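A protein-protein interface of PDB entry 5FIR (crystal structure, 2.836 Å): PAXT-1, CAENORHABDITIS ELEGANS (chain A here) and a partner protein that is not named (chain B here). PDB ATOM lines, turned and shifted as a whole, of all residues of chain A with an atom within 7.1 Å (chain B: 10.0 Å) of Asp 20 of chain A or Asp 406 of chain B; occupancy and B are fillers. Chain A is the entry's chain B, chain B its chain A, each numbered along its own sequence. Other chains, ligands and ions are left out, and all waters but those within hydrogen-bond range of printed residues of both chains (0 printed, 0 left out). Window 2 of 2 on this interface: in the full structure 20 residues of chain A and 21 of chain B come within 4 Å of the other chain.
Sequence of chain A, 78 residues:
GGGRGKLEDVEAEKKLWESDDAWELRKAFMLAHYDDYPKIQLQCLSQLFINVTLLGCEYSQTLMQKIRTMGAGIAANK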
ATOM      1  N   LYS A  14      15.483   4.843  -1.714  1.00  0.00           N
ATOM      2  CA  LYS A  14      16.080   3.681  -2.351  1.00  0.00           C
ATOM      3  C   LYS A  14      15.898   2.462  -1.463  1.00  0.00           C
ATOM      4  O   LYS A  14      15.938   2.558  -0.232  1.00  0.00           O
ATOM      5  CB  LYS A  14      17.569   3.925  -2.635  1.00  0.00           C
ATOM      6  CG  LYS A  14      18.214   2.856  -3.511  1.00  0.00           C
ATOM      7  CD  LYS A  14      19.748   2.899  -3.540  1.00  0.00           C
ATOM      8  CE  LYS A  14      20.318   1.705  -4.337  1.00  0.00           C
ATOM      9  NZ  LYS A  14      21.812   1.628  -4.349  1.00  0.00           N
ATOM     10  N   LEU A  16      17.458  -1.524  -1.011  1.00  0.00           N
ATOM     11  CA  LEU A  16      18.786  -2.087  -1.257  1.00  0.00           C
ATOM     12  C   LEU A  16      18.789  -3.101  -2.403  1.00  0.00           C
ATOM     13  O   LEU A  16      19.816  -3.290  -3.065  1.00  0.00           O
ATOM     14  CB  LEU A  16      19.313  -2.711   0.039  1.00  0.00           C
ATOM     15  CG  LEU A  16      19.872  -1.781   1.134  1.00  0.00           C
ATOM     16  CD1 LEU A  16      18.960  -0.593   1.541  1.00  0.00           C
ATOM     17  CD2 LEU A  16      20.246  -2.621   2.353  1.00  0.00           C
ATOM     18  N   TRP A  17      17.651  -3.744  -2.652  1.00  0.00           N
ATOM     19  CA  TRP A  17      17.410  -4.680  -3.747  1.00  0.00           C
ATOM     20  C   TRP A  17      17.195  -4.000  -5.109  1.00  0.00           C
ATOM     21  O   TRP A  17      17.170  -4.690  -6.139  1.00  0.00           O
ATOM     22  CB  TRP A  17      16.221  -5.573  -3.353  1.00  0.00           C
ATOM     23  CG  TRP A  17      15.023  -4.816  -2.799  1.00  0.00           C
ATOM     24  CD1 TRP A  17      14.824  -4.454  -1.493  1.00  0.00           C
ATOM     25  CD2 TRP A  17      13.848  -4.390  -3.516  1.00  0.00           C
ATOM     26  NE1 TRP A  17      13.624  -3.801  -1.364  1.00  0.00           N
ATOM     27  CE2 TRP A  17      12.999  -3.756  -2.586  1.00  0.00           C
ATOM     28  CE3 TRP A  17      13.438  -4.480  -4.845  1.00  0.00           C
ATOM     29  CZ2 TRP A  17      11.754  -3.206  -2.949  1.00  0.00           C
ATOM     30  CZ3 TRP A  17      12.194  -3.933  -5.204  1.00  0.00           C
ATOM     31  CH2 TRP A  17      11.376  -3.300  -4.259  1.00  0.00           C
ATOM     32  N   GLU A  18      17.046  -2.673  -5.136  1.00  0.00           N
ATOM     33  CA  GLU A  18      16.740  -1.949  -6.364  1.00  0.00           C
ATOM     34  C   GLU A  18      18.005  -1.911  -7.219  1.00  0.00           C
ATOM     35  O   GLU A  18      19.094  -1.601  -6.722  1.00  0.00           O
ATOM     36  CB  GLU A  18      16.245  -0.529  -6.035  1.00  0.00           C
ATOM     37  CG  GLU A  18      15.108   0.021  -6.925  1.00  0.00           C
ATOM     38  CD  GLU A  18      14.260   1.135  -6.265  1.00  0.00           C
ATOM     39  OE1 GLU A  18      14.421   1.399  -5.049  1.00  0.00           O
ATOM     40  OE2 GLU A  18      13.412   1.741  -6.967  1.00  0.00           O
ATOM     41  N   SER A  19      17.878  -2.268  -8.496  1.00  0.00           N
ATOM     42  CA  SER A  19      19.039  -2.166  -9.370  1.00  0.00           C
ATOM     43  C   SER A  19      19.491  -0.722  -9.471  1.00  0.00           C
ATOM     44  O   SER A  19      18.723   0.213  -9.246  1.00  0.00           O
ATOM     45  CB  SER A  19      18.705  -2.675 -10.775  1.00  0.00           C
ATOM     46  OG  SER A  19      19.645  -2.212 -11.729  1.00  0.00           O
ATOM     47  N   ASP A  20      20.758  -0.546  -9.847  1.00  0.00           N
ATOM     48  CA  ASP A  20      21.295   0.804  -9.916  1.00  0.00           C
ATOM     49  C   ASP A  20      20.644   1.576 -11.051  1.00  0.00           C
ATOM     50  O   ASP A  20      20.258   2.739 -10.882  1.00  0.00           O
ATOM     51  CB  ASP A  20      22.814   0.744 -10.029  1.00  0.00           C
ATOM     52  CG  ASP A  20      23.468   0.298  -8.717  1.00  0.00           C
ATOM     53  OD1 ASP A  20      22.719  -0.034  -7.765  1.00  0.00           O
ATOM     54  OD2 ASP A  20      24.720   0.266  -8.640  1.00  0.00           O
ATOM     55  N   ASP A  21      20.446   0.921 -12.193  1.00  0.00           N
ATOM     56  CA  ASP A  21      19.757   1.564 -13.308  1.00  0.00           C
ATOM     57  C   ASP A  21      18.295   1.840 -12.958  1.00  0.00           C
ATOM     58  O   ASP A  21      17.773   2.925 -13.231  1.00  0.00           O
ATOM     59  CB  ASP A  21      19.851   0.681 -14.550  1.00  0.00           C
ATOM     60  CG  ASP A  21      21.276   0.549 -15.066  1.00  0.00           C
ATOM     61  OD1 ASP A  21      22.042   1.541 -15.016  1.00  0.00           O
ATOM     62  OD2 ASP A  21      21.621  -0.558 -15.540  1.00  0.00           O
ATOM     63  N   ALA A  22      17.617   0.859 -12.360  1.00  0.00           N
ATOM     64  CA  ALA A  22      16.234   1.048 -11.945  1.00  0.00           C
ATOM     65  C   ALA A  22      16.108   2.092 -10.837  1.00  0.00           C
ATOM     66  O   ALA A  22      15.030   2.662 -10.640  1.00  0.00           O
ATOM     67  CB  ALA A  22      15.639  -0.283 -11.493  1.00  0.00           C
ATOM     68  N   TRP A  23      17.158   2.305 -10.051  1.00  0.00           N
ATOM     69  CA  TRP A  23      17.049   3.336  -9.036  1.00  0.00           C
ATOM     70  C   TRP A  23      17.107   4.708  -9.675  1.00  0.00           C
ATOM     71  O   TRP A  23      16.375   5.620  -9.278  1.00  0.00           O
ATOM     72  CB  TRP A  23      18.146   3.209  -7.993  1.00  0.00           C
ATOM     73  CG  TRP A  23      18.251   4.447  -7.157  1.00  0.00           C
ATOM     74  CD1 TRP A  23      19.352   5.223  -6.971  1.00  0.00           C
ATOM     75  CD2 TRP A  23      17.201   5.050  -6.392  1.00  0.00           C
ATOM     76  NE1 TRP A  23      19.054   6.271  -6.138  1.00  0.00           N
ATOM     77  CE2 TRP A  23      17.741   6.183  -5.765  1.00  0.00           C
ATOM     78  CE3 TRP A  23      15.859   4.745  -6.185  1.00  0.00           C
ATOM     79  CZ2 TRP A  23      16.989   7.003  -4.941  1.00  0.00           C
ATOM     80  CZ3 TRP A  23      15.116   5.564  -5.373  1.00  0.00           C
ATOM     81  CH2 TRP A  23      15.679   6.674  -4.755  1.00  0.00           C
ATOM     82  N   GLU A  24      17.989   4.884 -10.653  1.00  0.00           N
ATOM     83  CA  GLU A  24      18.100   6.195 -11.278  1.00  0.00           C
ATOM     84  C   GLU A  24      16.786   6.600 -11.934  1.00  0.00           C
ATOM     85  O   GLU A  24      16.384   7.766 -11.865  1.00  0.00           O
ATOM     86  CB  GLU A  24      19.250   6.211 -12.297  1.00  0.00           C
ATOM     87  CG  GLU A  24      20.675   6.178 -11.695  1.00  0.00           C
ATOM     88  CD  GLU A  24      21.082   7.476 -10.986  1.00  0.00           C
ATOM     89  OE1 GLU A  24      20.802   8.574 -11.520  1.00  0.00           O
ATOM     90  OE2 GLU A  24      21.688   7.394  -9.892  1.00  0.00           O
ATOM     91  N   LEU A  25      16.062   5.648 -12.512  1.00  0.00           N
ATOM     92  CA  LEU A  25      14.782   6.016 -13.085  1.00  0.00           C
ATOM     93  C   LEU A  25      13.818   6.474 -12.003  1.00  0.00           C
ATOM     94  O   LEU A  25      13.152   7.505 -12.150  1.00  0.00           O
ATOM     95  CB  LEU A  25      14.192   4.835 -13.840  1.00  0.00           C
ATOM     96  CG  LEU A  25      13.873   5.136 -15.304  1.00  0.00           C
ATOM     97  CD1 LEU A  25      14.932   4.510 -16.198  1.00  0.00           C
ATOM     98  CD2 LEU A  25      12.458   4.675 -15.683  1.00  0.00           C
ATOM     99  N   LYS B 392      25.624 -16.053 -18.489  1.00  0.00           N
ATOM    100  CA  LYS B 392      25.407 -15.419 -17.199  1.00  0.00           C
ATOM    101  C   LYS B 392      25.142 -13.924 -17.349  1.00  0.00           C
ATOM    102  O   LYS B 392      24.264 -13.377 -16.678  1.00  0.00           O
ATOM    103  CB  LYS B 392      26.609 -15.695 -16.301  1.00  0.00           C
ATOM    104  CG  LYS B 392      26.433 -15.378 -14.833  1.00  0.00           C
ATOM    105  CD  LYS B 392      27.333 -16.293 -14.015  1.00  0.00           C
ATOM    106  CE  LYS B 392      27.819 -15.602 -12.767  1.00  0.00           C
ATOM    107  NZ  LYS B 392      28.396 -16.555 -11.781  1.00  0.00           N
ATOM    108  N   ASP B 393      25.847 -13.252 -18.260  1.00  0.00           N
ATOM    109  CA  ASP B 393      25.697 -11.805 -18.346  1.00  0.00           C
ATOM    110  C   ASP B 393      24.399 -11.387 -19.023  1.00  0.00           C
ATOM    111  O   ASP B 393      23.764 -10.422 -18.580  1.00  0.00           O
ATOM    112  CB  ASP B 393      26.905 -11.222 -19.052  1.00  0.00           C
ATOM    113  CG  ASP B 393      28.183 -11.650 -18.392  1.00  0.00           C
ATOM    114  OD1 ASP B 393      28.613 -12.803 -18.642  1.00  0.00           O
ATOM    115  OD2 ASP B 393      28.724 -10.856 -17.590  1.00  0.00           O
ATOM    116  N   TYR B 396      21.707 -11.758 -16.335  1.00  0.00           N
ATOM    117  CA  TYR B 396      21.641 -10.680 -15.356  1.00  0.00           C
ATOM    118  C   TYR B 396      21.209  -9.380 -16.006  1.00  0.00           C
ATOM    119  O   TYR B 396      20.630  -8.525 -15.332  1.00  0.00           O
ATOM    120  CB  TYR B 396      22.972 -10.506 -14.625  1.00  0.00           C
ATOM    121  CG  TYR B 396      23.108 -11.375 -13.387  1.00  0.00           C
ATOM    122  CD1 TYR B 396      22.456 -11.036 -12.211  1.00  0.00           C
ATOM    123  CD2 TYR B 396      23.880 -12.532 -13.393  1.00  0.00           C
ATOM    124  CE1 TYR B 396      22.561 -11.813 -11.078  1.00  0.00           C
ATOM    125  CE2 TYR B 396      23.988 -13.323 -12.259  1.00  0.00           C
ATOM    126  CZ  TYR B 396      23.323 -12.950 -11.100  1.00  0.00           C
ATOM    127  OH  TYR B 396      23.416 -13.712  -9.954  1.00  0.00           O
ATOM    128  N   ARG B 397      21.470  -9.224 -17.310  1.00  0.00           N
ATOM    129  CA  ARG B 397      20.910  -8.102 -18.058  1.00  0.00           C
ATOM    130  C   ARG B 397      19.422  -8.312 -18.321  1.00  0.00           C
ATOM    131  O   ARG B 397      18.609  -7.401 -18.124  1.00  0.00           O
ATOM    132  CB  ARG B 397      21.677  -7.913 -19.371  1.00  0.00           C
ATOM    133  CG  ARG B 397      21.253  -6.696 -20.214  1.00  0.00           C
ATOM    134  CD  ARG B 397      22.257  -5.535 -20.112  1.00  0.00           C
ATOM    135  NE  ARG B 397      21.971  -4.620 -18.999  1.00  0.00           N
ATOM    136  CZ  ARG B 397      22.816  -3.685 -18.561  1.00  0.00           C
ATOM    137  NH1 ARG B 397      24.007  -3.541 -19.137  1.00  0.00           N
ATOM    138  NH2 ARG B 397      22.474  -2.897 -17.545  1.00  0.00           N
ATOM    139  N   PHE B 400      17.523  -8.816 -14.501  1.00  0.00           N
ATOM    140  CA  PHE B 400      17.688  -7.745 -13.516  1.00  0.00           C
ATOM    141  C   PHE B 400      18.088  -6.402 -14.118  1.00  0.00           C
ATOM    142  O   PHE B 400      18.039  -5.381 -13.411  1.00  0.00           O
ATOM    143  CB  PHE B 400      18.725  -8.122 -12.436  1.00  0.00           C
ATOM    144  CG  PHE B 400      18.370  -9.343 -11.630  1.00  0.00           C
ATOM    145  CD1 PHE B 400      17.341  -9.314 -10.721  1.00  0.00           C
ATOM    146  CD2 PHE B 400      19.119 -10.492 -11.729  1.00  0.00           C
ATOM    147  CE1 PHE B 400      17.014 -10.441  -9.972  1.00  0.00           C
ATOM    148  CE2 PHE B 400      18.810 -11.608 -10.971  1.00  0.00           C
ATOM    149  CZ  PHE B 400      17.757 -11.585 -10.099  1.00  0.00           C
ATOM    150  N   ASP B 401      18.478  -6.372 -15.393  1.00  0.00           N
ATOM    151  CA  ASP B 401      19.000  -5.185 -16.067  1.00  0.00           C
ATOM    152  C   ASP B 401      20.251  -4.666 -15.351  1.00  0.00           C
ATOM    153  O   ASP B 401      20.282  -3.566 -14.795  1.00  0.00           O
ATOM    154  CB  ASP B 401      17.919  -4.106 -16.199  1.00  0.00           C
ATOM    155  CG  ASP B 401      18.236  -3.092 -17.289  1.00  0.00           C
ATOM    156  OD1 ASP B 401      17.910  -3.362 -18.469  1.00  0.00           O
ATOM    157  OD2 ASP B 401      18.811  -2.028 -16.971  1.00  0.00           O
ATOM    158  N   VAL B 402      21.266  -5.537 -15.314  1.00  0.00           N
ATOM    159  CA  VAL B 402      22.615  -5.218 -14.858  1.00  0.00           C
ATOM    160  C   VAL B 402      23.575  -6.050 -15.704  1.00  0.00           C
ATOM    161  O   VAL B 402      23.185  -7.046 -16.315  1.00  0.00           O
ATOM    162  CB  VAL B 402      22.832  -5.493 -13.354  1.00  0.00           C
ATOM    163  CG1 VAL B 402      22.005  -4.551 -12.512  1.00  0.00           C
ATOM    164  CG2 VAL B 402      22.488  -6.915 -13.038  1.00  0.00           C
ATOM    165  N   GLY B 403      24.837  -5.620 -15.782  1.00  0.00           N
ATOM    166  CA  GLY B 403      25.707  -6.267 -16.744  1.00  0.00           C
ATOM    167  C   GLY B 403      27.205  -6.190 -16.515  1.00  0.00           C
ATOM    168  O   GLY B 403      27.800  -5.107 -16.582  1.00  0.00           O
ATOM    169  N   SER B 404      27.826  -7.352 -16.276  1.00  0.00           N
ATOM    170  CA  SER B 404      29.278  -7.544 -16.296  1.00  0.00           C
ATOM    171  C   SER B 404      30.014  -6.665 -15.291  1.00  0.00           C
ATOM    172  O   SER B 404      30.819  -7.165 -14.500  1.00  0.00           O
ATOM    173  CB  SER B 404      29.834  -7.262 -17.695  1.00  0.00           C
ATOM    174  OG  SER B 404      29.683  -8.381 -18.537  1.00  0.00           O
ATOM    175  N   ASP B 405      29.747  -5.357 -15.320  1.00  0.00           N
ATOM    176  CA  ASP B 405      30.408  -4.436 -14.403  1.00  0.00           C
ATOM    177  C   ASP B 405      30.030  -4.752 -12.959  1.00  0.00           C
ATOM    178  O   ASP B 405      30.889  -4.857 -12.077  1.00  0.00           O
ATOM    179  CB  ASP B 405      30.028  -2.998 -14.782  1.00  0.00           C
ATOM    180  CG  ASP B 405      30.677  -1.948 -13.891  1.00  0.00           C
ATOM    181  OD1 ASP B 405      31.856  -1.589 -14.133  1.00  0.00           O
ATOM    182  OD2 ASP B 405      29.988  -1.468 -12.960  1.00  0.00           O
ATOM    183  N   ASP B 406      28.738  -4.915 -12.708  1.00  0.00           N
ATOM    184  CA  ASP B 406      28.204  -5.032 -11.356  1.00  0.00           C
ATOM    185  C   ASP B 406      28.181  -6.492 -10.924  1.00  0.00           C
ATOM    186  O   ASP B 406      27.229  -7.215 -11.228  1.00  0.00           O
ATOM    187  CB  ASP B 406      26.808  -4.429 -11.293  1.00  0.00           C
ATOM    188  CG  ASP B 406      26.382  -4.108  -9.882  1.00  0.00           C
ATOM    189  OD1 ASP B 406      27.078  -4.558  -8.943  1.00  0.00           O
ATOM    190  OD2 ASP B 406      25.361  -3.400  -9.715  1.00  0.00           O
ATOM    191  N   ILE B 407      29.204  -6.939 -10.196  1.00  0.00           N
ATOM    192  CA  ILE B 407      29.082  -8.235  -9.535  1.00  0.00           C
ATOM    193  C   ILE B 407      28.840  -8.066  -8.049  1.00  0.00           C
ATOM    194  O   ILE B 407      28.643  -9.068  -7.347  1.00  0.00           O
ATOM    195  CB  ILE B 407      30.302  -9.157  -9.760  1.00  0.00           C
ATOM    196  CG1 ILE B 407      31.483  -8.735  -8.884  1.00  0.00           C
ATOM    197  CG2 ILE B 407      30.675  -9.184 -11.244  1.00  0.00           C
ATOM    198  CD1 ILE B 407      31.752  -9.715  -7.740  1.00  0.00           C
ATOM    199  N   GLU B 408      28.893  -6.836  -7.535  1.00  0.00           N
ATOM    200  CA  GLU B 408      28.337  -6.576  -6.216  1.00  0.00           C
ATOM    201  C   GLU B 408      26.856  -6.928  -6.179  1.00  0.00           C
ATOM    202  O   GLU B 408      26.347  -7.388  -5.150  1.00  0.00           O
ATOM    203  CB  GLU B 408      28.553  -5.110  -5.843  1.00  0.00           C
ATOM    204  CG  GLU B 408      27.839  -4.676  -4.570  1.00  0.00           C
ATOM    205  CD  GLU B 408      27.587  -3.175  -4.517  1.00  0.00           C
ATOM    206  OE1 GLU B 408      28.573  -2.399  -4.446  1.00  0.00           O
ATOM    207  OE2 GLU B 408      26.401  -2.772  -4.555  1.00  0.00           O
ATOM    208  N   PHE B 409      26.159  -6.740  -7.304  1.00  0.00           N
ATOM    209  CA  PHE B 409      24.745  -7.089  -7.383  1.00  0.00           C
ATOM    210  C   PHE B 409      24.558  -8.599  -7.377  1.00  0.00           C
ATOM    211  O   PHE B 409      23.721  -9.130  -6.640  1.00  0.00           O
ATOM    212  CB  PHE B 409      24.122  -6.476  -8.646  1.00  0.00           C
ATOM    213  CG  PHE B 409      22.657  -6.749  -8.786  1.00  0.00           C
ATOM    214  CD1 PHE B 409      21.728  -6.009  -8.067  1.00  0.00           C
ATOM    215  CD2 PHE B 409      22.205  -7.767  -9.606  1.00  0.00           C
ATOM    216  CE1 PHE B 409      20.369  -6.277  -8.167  1.00  0.00           C
ATOM    217  CE2 PHE B 409      20.846  -8.044  -9.712  1.00  0.00           C
ATOM    218  CZ  PHE B 409      19.926  -7.295  -8.992  1.00  0.00           C
ATOM    219  N   ARG B 410      25.348  -9.308  -8.177  1.00  0.00           N
ATOM    220  CA  ARG B 410      25.272 -10.762  -8.186  1.00  0.00           C
ATOM    221  C   ARG B 410      25.472 -11.323  -6.791  1.00  0.00           C
ATOM    222  O   ARG B 410      24.771 -12.257  -6.395  1.00  0.00           O
ATOM    223  CB  ARG B 410      26.297 -11.354  -9.154  1.00  0.00           C
ATOM    224  CG  ARG B 410      26.020 -11.021 -10.604  1.00  0.00           C
ATOM    225  CD  ARG B 410      27.114 -11.528 -11.518  1.00  0.00           C
ATOM    226  NE  ARG B 410      26.866 -11.139 -12.902  1.00  0.00           N
ATOM    227  CZ  ARG B 410      27.732 -11.323 -13.891  1.00  0.00           C
ATOM    228  NH1 ARG B 410      28.899 -11.905 -13.637  1.00  0.00           N
ATOM    229  NH2 ARG B 410      27.423 -10.946 -15.131  1.00  0.00           N
ATOM    230  N   HIS B 411      26.412 -10.772  -6.019  1.00  0.00           N
ATOM    231  CA  HIS B 411      26.544 -11.281  -4.659  1.00  0.00           C
ATOM    232  C   HIS B 411      25.374 -10.850  -3.783  1.00  0.00           C
ATOM    233  O   HIS B 411      24.966 -11.599  -2.887  1.00  0.00           O
ATOM    234  CB  HIS B 411      27.864 -10.833  -4.035  1.00  0.00           C
ATOM    235  CG  HIS B 411      29.072 -11.416  -4.698  1.00  0.00           C
ATOM    236  ND1 HIS B 411      30.357 -11.007  -4.403  1.00  0.00           N
ATOM    237  CD2 HIS B 411      29.190 -12.369  -5.654  1.00  0.00           C
ATOM    238  CE1 HIS B 411      31.213 -11.688  -5.144  1.00  0.00           C
ATOM    239  NE2 HIS B 411      30.531 -12.518  -5.914  1.00  0.00           N
ATOM    240  N   ARG B 412      24.750  -9.711  -4.092  1.00  0.00           N
ATOM    241  CA  ARG B 412      23.652  -9.244  -3.255  1.00  0.00           C
ATOM    242  C   ARG B 412      22.448 -10.185  -3.346  1.00  0.00           C
ATOM    243  O   ARG B 412      21.808 -10.470  -2.324  1.00  0.00           O
ATOM    244  CB  ARG B 412      23.297  -7.800  -3.615  1.00  0.00           C
ATOM    245  CG  ARG B 412      22.445  -7.132  -2.571  1.00  0.00           C
ATOM    246  CD  ARG B 412      22.251  -5.639  -2.790  1.00  0.00           C
ATOM    247  NE  ARG B 412      23.238  -4.816  -2.094  1.00  0.00           N
ATOM    248  CZ  ARG B 412      24.220  -4.145  -2.691  1.00  0.00           C
ATOM    249  NH1 ARG B 412      24.350  -4.184  -4.016  1.00  0.00           N
ATOM    250  NH2 ARG B 412      25.064  -3.421  -1.962  1.00  0.00           N
ATOM    251  N   VAL B 413      22.108 -10.668  -4.551  1.00  0.00           N
ATOM    252  CA  VAL B 413      21.015 -11.634  -4.644  1.00  0.00           C
ATOM    253  C   VAL B 413      21.440 -12.960  -4.022  1.00  0.00           C
ATOM    254  O   VAL B 413      20.669 -13.594  -3.292  1.00  0.00           O
ATOM    255  CB  VAL B 413      20.540 -11.837  -6.100  1.00  0.00           C
ATOM    256  CG1 VAL B 413      20.001 -10.566  -6.683  1.00  0.00           C
ATOM    257  CG2 VAL B 413      21.622 -12.381  -6.961  1.00  0.00           C
ATOM    258  N   TYR B 441      13.510 -10.452  -4.903  1.00  0.00           N
ATOM    259  CA  TYR B 441      13.838 -10.532  -6.320  1.00  0.00           C
ATOM    260  C   TYR B 441      12.881 -11.501  -6.992  1.00  0.00           C
ATOM    261  O   TYR B 441      12.301 -12.386  -6.356  1.00  0.00           O
ATOM    262  CB  TYR B 441      15.292 -10.993  -6.570  1.00  0.00           C
ATOM    263  CG  TYR B 441      16.332 -10.154  -5.877  1.00  0.00           C
ATOM    264  CD1 TYR B 441      16.818  -9.001  -6.461  1.00  0.00           C
ATOM    265  CD2 TYR B 441      16.823 -10.513  -4.633  1.00  0.00           C
ATOM    266  CE1 TYR B 441      17.769  -8.220  -5.810  1.00  0.00           C
ATOM    267  CE2 TYR B 441      17.760  -9.750  -3.977  1.00  0.00           C
ATOM    268  CZ  TYR B 441      18.237  -8.609  -4.561  1.00  0.00           C
ATOM    269  OH  TYR B 441      19.184  -7.854  -3.898  1.00  0.00           O
ATOM    270  N   ASP B 449      27.330 -17.768  -8.165  1.00  0.00           N
ATOM    271  CA  ASP B 449      27.296 -16.477  -7.486  1.00  0.00           C
ATOM    272  C   ASP B 449      27.447 -16.582  -5.972  1.00  0.00           C
ATOM    273  O   ASP B 449      27.631 -15.560  -5.296  1.00  0.00           O
ATOM    274  CB  ASP B 449      25.992 -15.761  -7.845  1.00  0.00           C
ATOM    275  CG  ASP B 449      25.866 -15.513  -9.353  1.00  0.00           C
ATOM    276  OD1 ASP B 449      26.860 -15.050  -9.971  1.00  0.00           O
ATOM    277  OD2 ASP B 449      24.796 -15.809  -9.927  1.00  0.00           O
ATOM    278  N   GLU B 451      29.855 -17.735  -4.183  1.00  0.00           N
ATOM    279  CA  GLU B 451      31.144 -17.506  -3.551  1.00  0.00           C
ATOM    280  C   GLU B 451      31.007 -16.383  -2.523  1.00  0.00           C
ATOM    281  O   GLU B 451      30.058 -15.586  -2.555  1.00  0.00           O
ATOM    282  CB  GLU B 451      32.191 -17.144  -4.591  1.00  0.00           C
ATOM    283  CG  GLU B 451      31.867 -15.840  -5.276  1.00  0.00           C
ATOM    284  CD  GLU B 451      32.316 -15.800  -6.713  1.00  0.00           C
ATOM    285  OE1 GLU B 451      33.301 -16.494  -7.037  1.00  0.00           O
ATOM    286  OE2 GLU B 451      31.699 -15.054  -7.510  1.00  0.00           O
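Printed residues of chain B within 4 Å of Trp 17 of chain A: Tyr 441.
Of the printed residues of chain B, Ser 19 of chain A touches Phe 400, Asp 401 and Val 402.
Of chain B, only Asp 406 (3.9 Å) comes within 4 Å of Asp 20 of chain A.
Ala 22 of chain A touches none of the printed residues of chain B.
Of the printed residues of chain A, Phe 400 of chain B touches Ser 19.
Printed residues of chain A within 4 Å of Asp 401 of chain B: Ser 19 (3.4 Å) and Asp 21 (3.4 Å).
Asp 406 of chain B touches just one residue of chain A: Asp 20.
Of the printed residues of chain A, Tyr 441 of chain B touches Trp 17 (3.6 Å).
The nearest residue of chain B that does not touch Asp 20 of chain A is Val 402 of chain B (5.0 Å).
The nearest printed residue of chain A that does not touch Phe 400 of chain B is Ala 22 of chain A (6.0 Å).
The side-chain amino group of Lys 14 of chain A is in salt-bridge range of the side-chain carboxylate of Asp 20 of chain A, 3.9 Å away.
OD1 of Asp 406 of chain B lies within hydrogen-bond range of N of Phe 409 of chain B, 2.9 Å away.
The guanidinium group (NH1) of Arg 412 of chain B lies within salt-bridge range of the side-chain carboxylate (OE2) of Glu 408 of chain B (2.5 Å).
The side-chain carboxylate (OD2) of Asp 401 of chain B is in salt-bridge range of the guanidinium group (NH2) of Arg 397 of chain B (3.8 Å).
The side-chain carboxylate (OD1) of Asp 406 of chain B sits at hydrogen-bond distance from the backbone NH (N) of Glu 408 of chain B (3.2 Å).
The side-chain hydroxyl (OG) of Ser 19 of chain A is in hydrogen-bond range of the backbone NH (N) of Asp 21 of chain A.
Of the 11 printed residues of chain A, 5 touch a printed residue of chain B.
Hydrophobic or aromatic side chains of chain A that line the printed part of chain B: Trp 17.
Of the 21 printed residues of chain B, 7 touch a printed residue of chain A.
Hydrophobic or aromatic side chains of chain B that line the printed part of chain A: Val 402 and Tyr 441.
Among the printed residues, 8 pairs touch across the chains.
OG of Ser 19 of chain A lies within hydrogen-bond range of O of Asp 401 of chain B, at 3.4 Å.
OD2 of Asp 21 of chain A is in salt-bridge range of NH2 of Arg 397 of chain B.
The side-chain carboxylate of Asp 21 of chain A lies close to the backbone carbonyl oxygen of Asp 401 of chain B (3.4 Å).
Among the printed residues, pairs that only touch across the chains: Leu 16 of chain A with Arg 412 of chain B, Trp 17 of chain A with Tyr 441 of chain B, Ser 19 of chain A with Phe 400 of chain B, Ser 19 of chain A with Val 402 of chain B and Asp 20 of chain A with Asp 406 of chain B.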
